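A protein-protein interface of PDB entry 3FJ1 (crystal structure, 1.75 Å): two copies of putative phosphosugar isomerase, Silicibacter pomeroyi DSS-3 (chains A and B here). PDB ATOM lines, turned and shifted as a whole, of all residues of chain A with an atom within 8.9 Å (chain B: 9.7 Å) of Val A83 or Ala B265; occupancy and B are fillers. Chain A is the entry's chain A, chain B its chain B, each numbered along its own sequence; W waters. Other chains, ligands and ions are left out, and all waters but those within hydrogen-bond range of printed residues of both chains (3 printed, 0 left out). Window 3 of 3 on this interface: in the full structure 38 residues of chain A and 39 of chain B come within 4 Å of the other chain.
Printed residues of chain A that touch a printed residue of chain B: Gly A77, Ser A79, Val A80, Ser A82, Val A83, Tyr A84, Ala A86 and Asp A106.
Hydrophobic or aromatic side chains of chain A within 4 Å of the printed part of chain B: Val A80, Val A83, Tyr A84 and Ala A86.
Of the 27 printed residues of chain B, 8 touch a printed residue of chain A.
Hydrophobic or aromatic side chains of chain B that line the printed part of chain A: Tyr B63, Leu B67, Ala B265 and Ala B266.
Among the printed residues, Asp or Glu carboxylates within 4 Å of a Lys or Arg side-chain nitrogen of the other chain: Asp A106 with Arg B213 (3.0 Å).
The side-chain hydroxyl (OG) of Ser A82 is in hydrogen-bond range of the side-chain carboxylate (OD1) of Asp A106 (3.2 Å).
OD1 of Asp B264 sits at hydrogen-bond distance from N of Ala B266.
OG of Ser B216 sits at hydrogen-bond distance from N of Arg B213, 3.0 Å away.
The backbone carbonyl oxygen (O) of Ser A79 lies within hydrogen-bond range of the backbone NH (N) of Tyr A84, at 3.0 Å.
The backbone carbonyl oxygen (O) of Val A80 is in hydrogen-bond range of the backbone NH (N) of Asp A85.
The side-chain carboxylate (OD1) of Asp B264 is in hydrogen-bond range of the backbone NH (N) of Glu B267, 3.4 Å away.
Water W1 lies within hydrogen-bond range of OD2 of Asp A106 (2.6 Å) and NH1 of Arg B213 (2.9 Å).
Water W2 lies within hydrogen-bond range of O of Arg B213, OD2 of Asp B264, N of Ser B216, OH of Tyr A84 and N of Thr B215.
Water W3 bridges OG of Ser A79 (2.8 Å) and OH of Tyr B63 (2.9 Å).
The side-chain hydroxyl (OH) of Tyr A84 is in hydrogen-bond range of the backbone NH (N) of Thr B215.
The side-chain carboxylate (OD2) of Asp A106 is in salt-bridge range of the guanidinium group (NH2) of Arg B213 (3.0 Å).
OH of Tyr A84 lies within hydrogen-bond range of OD2 of Asp B264, at 2.8 Å.
NH2 of Arg B213 sits at hydrogen-bond distance from OG of Ser A82, 3.4 Å away.
Among the printed residues, merely in contact across the chains: Gly A77 with Tyr B63, Ser A79 with Tyr B63, Ser A79 with Arg B213, Ser A79 with Gly B214, Val A80 with Tyr B63, Val A83 with Arg B213, Val A83 with Ala B265, Val A83 with Ala B266, Tyr A84 with Leu B67, Tyr A84 with Arg B213, Tyr A84 with Gly B214, Tyr A84 with Ala B266 and Ala A86 with Leu B67.
Ser A79 touches just these residues of chain B: Tyr B63, Arg B213 and Gly B214.
Ala A81 touches none of the printed residues of chain B.
Ser A82 touches just one residue of chain B: Arg B213 (3.4 Å).
Tyr A84 touches just these residues of chain B: Leu B67 (3.6 Å), Arg B213 (3.8 Å), Gly B214 (3.5 Å), Thr B215 (3.2 Å), Asp B264 (2.8 Å) and Ala B266 (3.8 Å).
Printed residues of chain B within 4 Å of Ala A86: Leu B67 (3.8 Å).
Printed residues of chain A within 4 Å of Tyr B63: Gly A77, Ser A79 and Val A80.
Asp B264 touches one residue of chain A.
Of chain A, only Val A83 comes within 4 Å of Ala B265.
Ala B266 touches just these residues of chain A: Val A83 (3.5 Å) and Tyr A84 (3.8 Å).
The nearest residue of chain A that does not touch Ala B265 is Tyr A84 (4.1 Å).
No position is printed for both chains.
Of the 17 pairs that touch across the chains among the printed residues, none has its exchanged pair printed and touching as well.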
ATOM      1  N   GLY A  77     -21.301  12.186  -3.955  1.00  0.00           N
ATOM      2  CA  GLY A  77     -19.853  12.206  -3.908  1.00  0.00           C
ATOM      3  C   GLY A  77     -19.363  13.358  -4.768  1.00  0.00           C
ATOM      4  O   GLY A  77     -19.668  13.374  -5.960  1.00  0.00           O
ATOM      5  N   PRO A  78     -18.617  14.330  -4.189  1.00  0.00           N
ATOM      6  CA  PRO A  78     -18.254  15.511  -5.014  1.00  0.00           C
ATOM      7  C   PRO A  78     -17.477  15.224  -6.277  1.00  0.00           C
ATOM      8  O   PRO A  78     -17.515  16.027  -7.195  1.00  0.00           O
ATOM      9  CB  PRO A  78     -17.493  16.416  -4.040  1.00  0.00           C
ATOM     10  CG  PRO A  78     -17.972  15.979  -2.631  1.00  0.00           C
ATOM     11  CD  PRO A  78     -18.150  14.484  -2.787  1.00  0.00           C
ATOM     12  N   SER A  79     -16.809  14.065  -6.348  1.00  0.00           N
ATOM     13  CA  SER A  79     -16.080  13.690  -7.582  1.00  0.00           C
ATOM     14  C   SER A  79     -17.002  13.589  -8.792  1.00  0.00           C
ATOM     15  O   SER A  79     -16.558  13.804  -9.930  1.00  0.00           O
ATOM     16  CB  SER A  79     -15.301  12.387  -7.409  1.00  0.00           C
ATOM     17  OG  SER A  79     -16.137  11.224  -7.304  1.00  0.00           O
ATOM     18  N   VAL A  80     -18.279  13.295  -8.549  1.00  0.00           N
ATOM     19  CA  VAL A  80     -19.268  13.207  -9.634  1.00  0.00           C
ATOM     20  C   VAL A  80     -19.274  14.496 -10.461  1.00  0.00           C
ATOM     21  O   VAL A  80     -19.435  14.466 -11.686  1.00  0.00           O
ATOM     22  CB  VAL A  80     -20.656  12.816  -9.103  1.00  0.00           C
ATOM     23  CG1 VAL A  80     -21.699  12.911 -10.190  1.00  0.00           C
ATOM     24  CG2 VAL A  80     -20.609  11.365  -8.557  1.00  0.00           C
ATOM     25  N   ALA A  81     -19.076  15.620  -9.775  1.00  0.00           N
ATOM     26  CA  ALA A  81     -18.932  16.915 -10.451  1.00  0.00           C
ATOM     27  C   ALA A  81     -17.477  17.244 -10.782  1.00  0.00           C
ATOM     28  O   ALA A  81     -17.130  17.568 -11.938  1.00  0.00           O
ATOM     29  CB  ALA A  81     -19.514  18.031  -9.603  1.00  0.00           C
ATOM     30  N   SER A  82     -16.625  17.184  -9.765  1.00  0.00           N
ATOM     31  CA  SER A  82     -15.243  17.711  -9.882  1.00  0.00           C
ATOM     32  C   SER A  82     -14.300  16.873 -10.736  1.00  0.00           C
ATOM     33  O   SER A  82     -13.325  17.406 -11.294  1.00  0.00           O
ATOM     34  CB  SER A  82     -14.627  17.927  -8.489  1.00  0.00           C
ATOM     35  OG  SER A  82     -14.326  16.680  -7.884  1.00  0.00           O
ATOM     36  N   VAL A  83     -14.556  15.569 -10.817  1.00  0.00           N
ATOM     37  CA  VAL A  83     -13.754  14.688 -11.658  1.00  0.00           C
ATOM     38  C   VAL A  83     -14.491  14.336 -12.950  1.00  0.00           C
ATOM     39  O   VAL A  83     -13.957  14.515 -14.048  1.00  0.00           O
ATOM     40  CB  VAL A  83     -13.313  13.412 -10.869  1.00  0.00           C
ATOM     41  CG1 VAL A  83     -12.611  12.417 -11.783  1.00  0.00           C
ATOM     42  CG2 VAL A  83     -12.415  13.809  -9.699  1.00  0.00           C
ATOM     43  N   TYR A  84     -15.725  13.862 -12.841  1.00  0.00           N
ATOM     44  CA  TYR A  84     -16.461  13.369 -14.017  1.00  0.00           C
ATOM     45  C   TYR A  84     -17.341  14.401 -14.725  1.00  0.00           C
ATOM     46  O   TYR A  84     -17.734  14.181 -15.877  1.00  0.00           O
ATOM     47  CB  TYR A  84     -17.348  12.190 -13.620  1.00  0.00           C
ATOM     48  CG  TYR A  84     -16.589  11.056 -12.978  1.00  0.00           C
ATOM     49  CD1 TYR A  84     -15.882  10.127 -13.749  1.00  0.00           C
ATOM     50  CD2 TYR A  84     -16.552  10.933 -11.607  1.00  0.00           C
ATOM     51  CE1 TYR A  84     -15.186   9.090 -13.142  1.00  0.00           C
ATOM     52  CE2 TYR A  84     -15.869   9.891 -10.990  1.00  0.00           C
ATOM     53  CZ  TYR A  84     -15.182   8.985 -11.764  1.00  0.00           C
ATOM     54  OH  TYR A  84     -14.530   7.970 -11.136  1.00  0.00           O
ATOM     55  N   ASP A  85     -17.659  15.489 -14.026  1.00  0.00           N
ATOM     56  CA  ASP A  85     -18.605  16.505 -14.505  1.00  0.00           C
ATOM     57  C   ASP A  85     -19.835  15.844 -15.135  1.00  0.00           C
ATOM     58  O   ASP A  85     -20.219  16.174 -16.254  1.00  0.00           O
ATOM     59  CB  ASP A  85     -17.933  17.455 -15.502  1.00  0.00           C
ATOM     60  CG  ASP A  85     -18.761  18.687 -15.797  1.00  0.00           C
ATOM     61  OD1 ASP A  85     -19.618  19.077 -14.976  1.00  0.00           O
ATOM     62  OD2 ASP A  85     -18.508  19.277 -16.874  1.00  0.00           O
ATOM     63  N   ALA A  86     -20.438  14.900 -14.416  1.00  0.00           N
ATOM     64  CA  ALA A  86     -21.615  14.217 -14.878  1.00  0.00           C
ATOM     65  C   ALA A  86     -22.825  15.147 -14.806  1.00  0.00           C
ATOM     66  O   ALA A  86     -22.915  16.067 -13.950  1.00  0.00           O
ATOM     67  CB  ALA A  86     -21.859  12.916 -14.052  1.00  0.00           C
ATOM     68  N   PRO A 105     -12.959  23.425  -3.186  1.00  0.00           N
ATOM     69  CA  PRO A 105     -13.315  23.379  -4.592  1.00  0.00           C
ATOM     70  C   PRO A 105     -14.269  22.240  -4.962  1.00  0.00           C
ATOM     71  O   PRO A 105     -15.133  22.435  -5.797  1.00  0.00           O
ATOM     72  CB  PRO A 105     -11.957  23.221  -5.296  1.00  0.00           C
ATOM     73  CG  PRO A 105     -10.974  23.815  -4.335  1.00  0.00           C
ATOM     74  CD  PRO A 105     -11.499  23.492  -2.988  1.00  0.00           C
ATOM     75  N   ASP A 106     -14.088  21.060  -4.376  1.00  0.00           N
ATOM     76  CA  ASP A 106     -14.986  19.943  -4.644  1.00  0.00           C
ATOM     77  C   ASP A 106     -16.425  20.215  -4.205  1.00  0.00           C
ATOM     78  O   ASP A 106     -17.361  19.939  -4.940  1.00  0.00           O
ATOM     79  CB  ASP A 106     -14.475  18.662  -3.984  1.00  0.00           C
ATOM     80  CG  ASP A 106     -13.292  18.055  -4.712  1.00  0.00           C
ATOM     81  OD1 ASP A 106     -12.848  18.604  -5.752  1.00  0.00           O
ATOM     82  OD2 ASP A 106     -12.797  17.029  -4.211  1.00  0.00           O
ATOM     83  N   ALA A 109     -17.882  22.802  -6.514  1.00  0.00           N
ATOM     84  CA  ALA A 109     -18.160  22.228  -7.832  1.00  0.00           C
ATOM     85  C   ALA A 109     -19.433  21.389  -7.856  1.00  0.00           C
ATOM     86  O   ALA A 109     -20.208  21.482  -8.794  1.00  0.00           O
ATOM     87  CB  ALA A 109     -16.991  21.408  -8.347  1.00  0.00           C
ATOM     88  N   MET A 110     -19.615  20.557  -6.839  1.00  0.00           N
ATOM     89  CA  MET A 110     -20.766  19.694  -6.762  1.00  0.00           C
ATOM     90  C   MET A 110     -22.028  20.544  -6.562  1.00  0.00           C
ATOM     91  O   MET A 110     -23.069  20.304  -7.217  1.00  0.00           O
ATOM     92  CB  MET A 110     -20.561  18.670  -5.656  1.00  0.00           C
ATOM     93  CG  MET A 110     -21.618  17.612  -5.562  1.00  0.00           C
ATOM     94  SD  MET A 110     -21.691  16.319  -7.051  1.00  0.00           S
ATOM     95  CE  MET A 110     -23.061  17.334  -7.913  1.00  0.00           C
ATOM     96  N   ASN A 113     -22.797  22.370  -9.868  1.00  0.00           N
ATOM     97  CA  ASN A 113     -23.361  21.427 -10.836  1.00  0.00           C
ATOM     98  C   ASN A 113     -24.787  21.047 -10.486  1.00  0.00           C
ATOM     99  O   ASN A 113     -25.646  20.883 -11.375  1.00  0.00           O
ATOM    100  CB  ASN A 113     -22.488  20.156 -10.970  1.00  0.00           C
ATOM    101  CG  ASN A 113     -21.291  20.358 -11.927  1.00  0.00           C
ATOM    102  OD1 ASN A 113     -20.903  21.507 -12.234  1.00  0.00           O
ATOM    103  ND2 ASN A 113     -20.686  19.248 -12.376  1.00  0.00           N
ATOM    104  N   TYR B  63     -22.192   5.130  -8.029  1.00  0.00           N
ATOM    105  CA  TYR B  63     -21.339   5.832  -9.010  1.00  0.00           C
ATOM    106  C   TYR B  63     -21.721   5.424 -10.438  1.00  0.00           C
ATOM    107  O   TYR B  63     -21.901   6.269 -11.301  1.00  0.00           O
ATOM    108  CB  TYR B  63     -19.858   5.543  -8.751  1.00  0.00           C
ATOM    109  CG  TYR B  63     -19.296   6.426  -7.678  1.00  0.00           C
ATOM    110  CD1 TYR B  63     -18.991   7.743  -7.947  1.00  0.00           C
ATOM    111  CD2 TYR B  63     -19.086   5.959  -6.397  1.00  0.00           C
ATOM    112  CE1 TYR B  63     -18.472   8.581  -6.975  1.00  0.00           C
ATOM    113  CE2 TYR B  63     -18.559   6.792  -5.405  1.00  0.00           C
ATOM    114  CZ  TYR B  63     -18.285   8.097  -5.690  1.00  0.00           C
ATOM    115  OH  TYR B  63     -17.766   8.912  -4.715  1.00  0.00           O
ATOM    116  N   LEU B  67     -23.132   8.114 -13.229  1.00  0.00           N
ATOM    117  CA  LEU B  67     -22.284   8.377 -14.395  1.00  0.00           C
ATOM    118  C   LEU B  67     -22.928   7.903 -15.705  1.00  0.00           C
ATOM    119  O   LEU B  67     -22.812   8.600 -16.731  1.00  0.00           O
ATOM    120  CB  LEU B  67     -20.887   7.731 -14.213  1.00  0.00           C
ATOM    121  CG  LEU B  67     -20.045   8.226 -13.029  1.00  0.00           C
ATOM    122  CD1 LEU B  67     -18.670   7.512 -12.965  1.00  0.00           C
ATOM    123  CD2 LEU B  67     -19.927   9.744 -13.046  1.00  0.00           C
ATOM    124  N   GLY B 212      -9.146   5.279  -3.009  1.00  0.00           N
ATOM    125  CA  GLY B 212      -9.881   5.281  -4.245  1.00  0.00           C
ATOM    126  C   GLY B 212     -10.307   6.710  -4.520  1.00  0.00           C
ATOM    127  O   GLY B 212     -10.155   7.589  -3.670  1.00  0.00           O
ATOM    128  N   ARG B 213     -10.812   6.932  -5.716  1.00  0.00           N
ATOM    129  CA  ARG B 213     -11.261   8.267  -6.129  1.00  0.00           C
ATOM    130  C   ARG B 213     -12.411   8.072  -7.110  1.00  0.00           C
ATOM    131  O   ARG B 213     -12.240   7.477  -8.150  1.00  0.00           O
ATOM    132  CB  ARG B 213     -10.138   9.025  -6.811  1.00  0.00           C
ATOM    133  CG  ARG B 213     -10.455  10.500  -7.207  1.00  0.00           C
ATOM    134  CD  ARG B 213     -10.992  11.317  -6.022  1.00  0.00           C
ATOM    135  NE  ARG B 213     -11.168  12.739  -6.357  1.00  0.00           N
ATOM    136  CZ  ARG B 213     -11.970  13.579  -5.699  1.00  0.00           C
ATOM    137  NH1 ARG B 213     -12.712  13.155  -4.707  1.00  0.00           N
ATOM    138  NH2 ARG B 213     -12.051  14.849  -6.062  1.00  0.00           N
ATOM    139  N   GLY B 214     -13.598   8.555  -6.775  1.00  0.00           N
ATOM    140  CA  GLY B 214     -14.737   8.288  -7.625  1.00  0.00           C
ATOM    141  C   GLY B 214     -15.138   6.821  -7.530  1.00  0.00           C
ATOM    142  O   GLY B 214     -15.115   6.257  -6.471  1.00  0.00           O
ATOM    143  N   THR B 215     -15.479   6.207  -8.653  1.00  0.00           N
ATOM    144  CA  THR B 215     -15.980   4.849  -8.656  1.00  0.00           C
ATOM    145  C   THR B 215     -15.110   3.868  -7.900  1.00  0.00           C
ATOM    146  O   THR B 215     -15.629   3.057  -7.167  1.00  0.00           O
ATOM    147  CB  THR B 215     -16.212   4.361 -10.094  1.00  0.00           C
ATOM    148  OG1 THR B 215     -16.966   5.364 -10.794  1.00  0.00           O
ATOM    149  CG2 THR B 215     -16.932   3.009 -10.111  1.00  0.00           C
ATOM    150  N   SER B 216     -13.784   3.977  -8.047  1.00  0.00           N
ATOM    151  CA  SER B 216     -12.866   3.026  -7.411  1.00  0.00           C
ATOM    152  C   SER B 216     -12.872   3.073  -5.874  1.00  0.00           C
ATOM    153  O   SER B 216     -12.362   2.184  -5.245  1.00  0.00           O
ATOM    154  CB  SER B 216     -11.442   3.241  -7.928  1.00  0.00           C
ATOM    155  OG  SER B 216     -10.893   4.421  -7.379  1.00  0.00           O
ATOM    156  N   SER B 239     -10.784   8.331   0.475  1.00  0.00           N
ATOM    157  CA  SER B 239     -10.752   8.983  -0.809  1.00  0.00           C
ATOM    158  C   SER B 239      -9.354   9.598  -0.904  1.00  0.00           C
ATOM    159  O   SER B 239      -8.860  10.189   0.083  1.00  0.00           O
ATOM    160  CB  SER B 239     -11.780  10.124  -0.863  1.00  0.00           C
ATOM    161  OG  SER B 239     -11.551  10.932  -2.002  1.00  0.00           O
ATOM    162  N   SER B 240      -8.707   9.470  -2.066  1.00  0.00           N
ATOM    163  CA  SER B 240      -7.436  10.145  -2.303  1.00  0.00           C
ATOM    164  C   SER B 240      -7.547  11.652  -2.110  1.00  0.00           C
ATOM    165  O   SER B 240      -6.570  12.287  -1.777  1.00  0.00           O
ATOM    166  CB  SER B 240      -6.882   9.851  -3.708  1.00  0.00           C
ATOM    167  OG  SER B 240      -7.790  10.139  -4.786  1.00  0.00           O
ATOM    168  N   ALA B 241      -8.721  12.238  -2.365  1.00  0.00           N
ATOM    169  CA  ALA B 241      -8.921  13.685  -2.187  1.00  0.00           C
ATOM    170  C   ALA B 241      -9.034  14.104  -0.721  1.00  0.00           C
ATOM    171  O   ALA B 241      -9.034  15.315  -0.423  1.00  0.00           O
ATOM    172  CB  ALA B 241     -10.151  14.181  -2.954  1.00  0.00           C
ATOM    173  N   ALA B 261      -6.898   2.551  -8.823  1.00  0.00           N
ATOM    174  CA  ALA B 261      -7.181   3.420  -9.963  1.00  0.00           C
ATOM    175  C   ALA B 261      -7.750   2.608 -11.123  1.00  0.00           C
ATOM    176  O   ALA B 261      -7.139   1.650 -11.565  1.00  0.00           O
ATOM    177  CB  ALA B 261      -5.883   4.137 -10.431  1.00  0.00           C
ATOM    178  N   ALA B 262      -8.934   2.982 -11.573  1.00  0.00           N
ATOM    179  CA  ALA B 262      -9.579   2.475 -12.788  1.00  0.00           C
ATOM    180  C   ALA B 262      -9.097   3.363 -13.930  1.00  0.00           C
ATOM    181  O   ALA B 262      -8.472   4.397 -13.698  1.00  0.00           O
ATOM    182  CB  ALA B 262     -11.108   2.614 -12.659  1.00  0.00           C
ATOM    183  N   GLY B 263      -9.372   2.937 -15.166  1.00  0.00           N
ATOM    184  CA  GLY B 263      -9.041   3.676 -16.370  1.00  0.00           C
ATOM    185  C   GLY B 263     -10.109   4.691 -16.704  1.00  0.00           C
ATOM    186  O   GLY B 263     -10.727   4.629 -17.765  1.00  0.00           O
ATOM    187  N   ASP B 264     -10.332   5.623 -15.777  1.00  0.00           N
ATOM    188  CA  ASP B 264     -11.357   6.649 -15.897  1.00  0.00           C
ATOM    189  C   ASP B 264     -10.744   8.008 -15.606  1.00  0.00           C
ATOM    190  O   ASP B 264      -9.520   8.138 -15.489  1.00  0.00           O
ATOM    191  CB  ASP B 264     -12.571   6.346 -15.000  1.00  0.00           C
ATOM    192  CG  ASP B 264     -12.254   6.385 -13.509  1.00  0.00           C
ATOM    193  OD1 ASP B 264     -11.088   6.718 -13.124  1.00  0.00           O
ATOM    194  OD2 ASP B 264     -13.204   6.105 -12.706  1.00  0.00           O
ATOM    195  N   ALA B 265     -11.596   9.022 -15.487  1.00  0.00           N
ATOM    196  CA  ALA B 265     -11.150  10.398 -15.232  1.00  0.00           C
ATOM    197  C   ALA B 265     -10.490  10.601 -13.875  1.00  0.00           C
ATOM    198  O   ALA B 265      -9.826  11.623 -13.658  1.00  0.00           O
ATOM    199  CB  ALA B 265     -12.322  11.363 -15.375  1.00  0.00           C
ATOM    200  N   ALA B 266     -10.708   9.669 -12.947  1.00  0.00           N
ATOM    201  CA  ALA B 266     -10.086   9.716 -11.608  1.00  0.00           C
ATOM    202  C   ALA B 266      -8.682   9.116 -11.547  1.00  0.00           C
ATOM    203  O   ALA B 266      -8.027   9.237 -10.507  1.00  0.00           O
ATOM    204  CB  ALA B 266     -10.952   8.992 -10.579  1.00  0.00           C
ATOM    205  N   GLU B 267      -8.220   8.502 -12.640  1.00  0.00           N
ATOM    206  CA  GLU B 267      -6.899   7.862 -12.658  1.00  0.00           C
ATOM    207  C   GLU B 267      -5.774   8.869 -12.396  1.00  0.00           C
ATOM    208  O   GLU B 267      -4.913   8.643 -11.549  1.00  0.00           O
ATOM    209  CB  GLU B 267      -6.657   7.128 -13.974  1.00  0.00           C
ATOM    210  CG  GLU B 267      -5.347   6.335 -13.970  1.00  0.00           C
ATOM    211  CD  GLU B 267      -5.136   5.454 -15.170  1.00  0.00           C
ATOM    212  OE1 GLU B 267      -5.908   5.597 -16.174  1.00  0.00           O
ATOM    213  OE2 GLU B 267      -4.162   4.655 -15.121  1.00  0.00           O
ATOM    214  N   ALA B 268      -5.816   9.998 -13.093  1.00  0.00           N
ATOM    215  CA  ALA B 268      -4.769  11.007 -12.960  1.00  0.00           C
ATOM    216  C   ALA B 268      -4.729  11.613 -11.549  1.00  0.00           C
ATOM    217  O   ALA B 268      -3.647  11.689 -10.946  1.00  0.00           O
ATOM    218  CB  ALA B 268      -4.939  12.098 -14.055  1.00  0.00           C
ATOM    219  N   PRO B 269      -5.872  12.092 -11.025  1.00  0.00           N
ATOM    220  CA  PRO B 269      -5.826  12.601  -9.649  1.00  0.00           C
ATOM    221  C   PRO B 269      -5.422  11.577  -8.570  1.00  0.00           C
ATOM    222  O   PRO B 269      -4.767  11.940  -7.587  1.00  0.00           O
ATOM    223  CB  PRO B 269      -7.233  13.140  -9.419  1.00  0.00           C
ATOM    224  CG  PRO B 269      -8.076  12.564 -10.466  1.00  0.00           C
ATOM    225  CD  PRO B 269      -7.172  12.358 -11.661  1.00  0.00           C
ATOM    226  N   LEU B 270      -5.765  10.321  -8.767  1.00  0.00           N
ATOM    227  CA  LEU B 270      -5.351   9.270  -7.837  1.00  0.00           C
ATOM    228  C   LEU B 270      -3.841   9.096  -7.883  1.00  0.00           C
ATOM    229  O   LEU B 270      -3.180   9.077  -6.851  1.00  0.00           O
ATOM    230  CB  LEU B 270      -6.085   7.961  -8.188  1.00  0.00           C
ATOM    231  CG  LEU B 270      -5.880   6.705  -7.308  1.00  0.00           C
ATOM    232  CD1 LEU B 270      -4.457   6.107  -7.395  1.00  0.00           C
ATOM    233  CD2 LEU B 270      -6.278   6.965  -5.888  1.00  0.00           C
ATOM    234  N   ALA B 271      -3.298   9.027  -9.089  1.00  0.00           N
ATOM    235  CA  ALA B 271      -1.865   8.869  -9.292  1.00  0.00           C
ATOM    236  C   ALA B 271      -1.076  10.051  -8.708  1.00  0.00           C
ATOM    237  O   ALA B 271      -0.017   9.846  -8.126  1.00  0.00           O
ATOM    238  CB  ALA B 271      -1.564   8.714 -10.787  1.00  0.00           C
ATOM    239  N   GLU B 272      -1.581  11.278  -8.890  1.00  0.00           N
ATOM    240  CA  GLU B 272      -0.962  12.489  -8.327  1.00  0.00           C
ATOM    241  C   GLU B 272      -0.888  12.428  -6.790  1.00  0.00           C
ATOM    242  O   GLU B 272       0.179  12.660  -6.200  1.00  0.00           O
ATOM    243  CB  GLU B 272      -1.725  13.746  -8.778  1.00  0.00           C
ATOM    244  N   ARG B 301      -6.595  -4.317 -17.235  1.00  0.00           N
ATOM    245  CA  ARG B 301      -7.728  -3.442 -17.610  1.00  0.00           C
ATOM    246  C   ARG B 301      -8.806  -4.283 -18.288  1.00  0.00           C
ATOM    247  O   ARG B 301      -8.496  -5.339 -18.865  1.00  0.00           O
ATOM    248  CB  ARG B 301      -7.270  -2.236 -18.461  1.00  0.00           C
ATOM    249  CG  ARG B 301      -6.460  -1.233 -17.681  1.00  0.00           C
ATOM    250  CD  ARG B 301      -7.370  -0.327 -16.858  1.00  0.00           C
ATOM    251  NE  ARG B 301      -6.624   0.738 -16.201  1.00  0.00           N
ATOM    252  CZ  ARG B 301      -6.428   0.878 -14.895  1.00  0.00           C
ATOM    253  NH1 ARG B 301      -6.943   0.035 -13.994  1.00  0.00           N
ATOM    254  NH2 ARG B 301      -5.706   1.924 -14.480  1.00  0.00           N
ATOM    255  N   HIS B 304     -13.724  -1.394 -20.114  1.00  0.00           N
ATOM    256  CA  HIS B 304     -14.593  -0.295 -19.730  1.00  0.00           C
ATOM    257  C   HIS B 304     -14.211   0.207 -18.341  1.00  0.00           C
ATOM    258  O   HIS B 304     -13.909  -0.605 -17.460  1.00  0.00           O
ATOM    259  CB  HIS B 304     -16.082  -0.690 -19.774  1.00  0.00           C
ATOM    260  CG  HIS B 304     -17.000   0.493 -19.780  1.00  0.00           C
ATOM    261  ND1 HIS B 304     -17.248   1.234 -18.652  1.00  0.00           N
ATOM    262  CD2 HIS B 304     -17.665   1.113 -20.791  1.00  0.00           C
ATOM    263  CE1 HIS B 304     -18.076   2.222 -18.946  1.00  0.00           C
ATOM    264  NE2 HIS B 304     -18.345   2.174 -20.240  1.00  0.00           N
ATOM    265  N   ALA B 305     -14.254   1.542 -18.174  1.00  0.00           N
ATOM    266  CA  ALA B 305     -13.939   2.207 -16.891  1.00  0.00           C
ATOM    267  C   ALA B 305     -14.705   1.575 -15.731  1.00  0.00           C
ATOM    268  O   ALA B 305     -14.168   1.381 -14.643  1.00  0.00           O
ATOM    269  CB  ALA B 305     -14.323   3.692 -16.957  1.00  0.00           C
ATOM    270  N   LEU B 306     -15.977   1.281 -15.963  1.00  0.00           N
ATOM    271  CA  LEU B 306     -16.839   0.824 -14.884  1.00  0.00           C
ATOM    272  C   LEU B 306     -16.600  -0.612 -14.462  1.00  0.00           C
ATOM    273  O   LEU B 306     -16.979  -0.976 -13.356  1.00  0.00           O
ATOM    274  CB  LEU B 306     -18.300   1.075 -15.193  1.00  0.00           C
ATOM    275  CG  LEU B 306     -18.793   2.545 -15.353  1.00  0.00           C
ATOM    276  CD1 LEU B 306     -20.290   2.596 -15.791  1.00  0.00           C
ATOM    277  CD2 LEU B 306     -18.596   3.295 -14.037  1.00  0.00           C
ATOM    278  N   ASP B 308     -13.367  -1.968 -14.652  1.00  0.00           N
ATOM    279  CA  ASP B 308     -11.983  -1.988 -14.188  1.00  0.00           C
ATOM    280  C   ASP B 308     -11.834  -2.319 -12.702  1.00  0.00           C
ATOM    281  O   ASP B 308     -10.972  -3.083 -12.361  1.00  0.00           O
ATOM    282  CB  ASP B 308     -11.248  -0.687 -14.531  1.00  0.00           C
ATOM    283  CG  ASP B 308     -10.833  -0.608 -16.011  1.00  0.00           C
ATOM    284  OD1 ASP B 308     -10.913  -1.636 -16.752  1.00  0.00           O
ATOM    285  OD2 ASP B 308     -10.411   0.506 -16.407  1.00  0.00           O
HETATM  286  O   HOH W   1     -14.317  15.181  -3.299  1.00  0.00           O
HETATM  287  O   HOH W   2     -12.488   5.594 -10.044  1.00  0.00           O
HETATM  288  O   HOH W   3     -16.544  11.561  -4.550  1.00  0.00           O
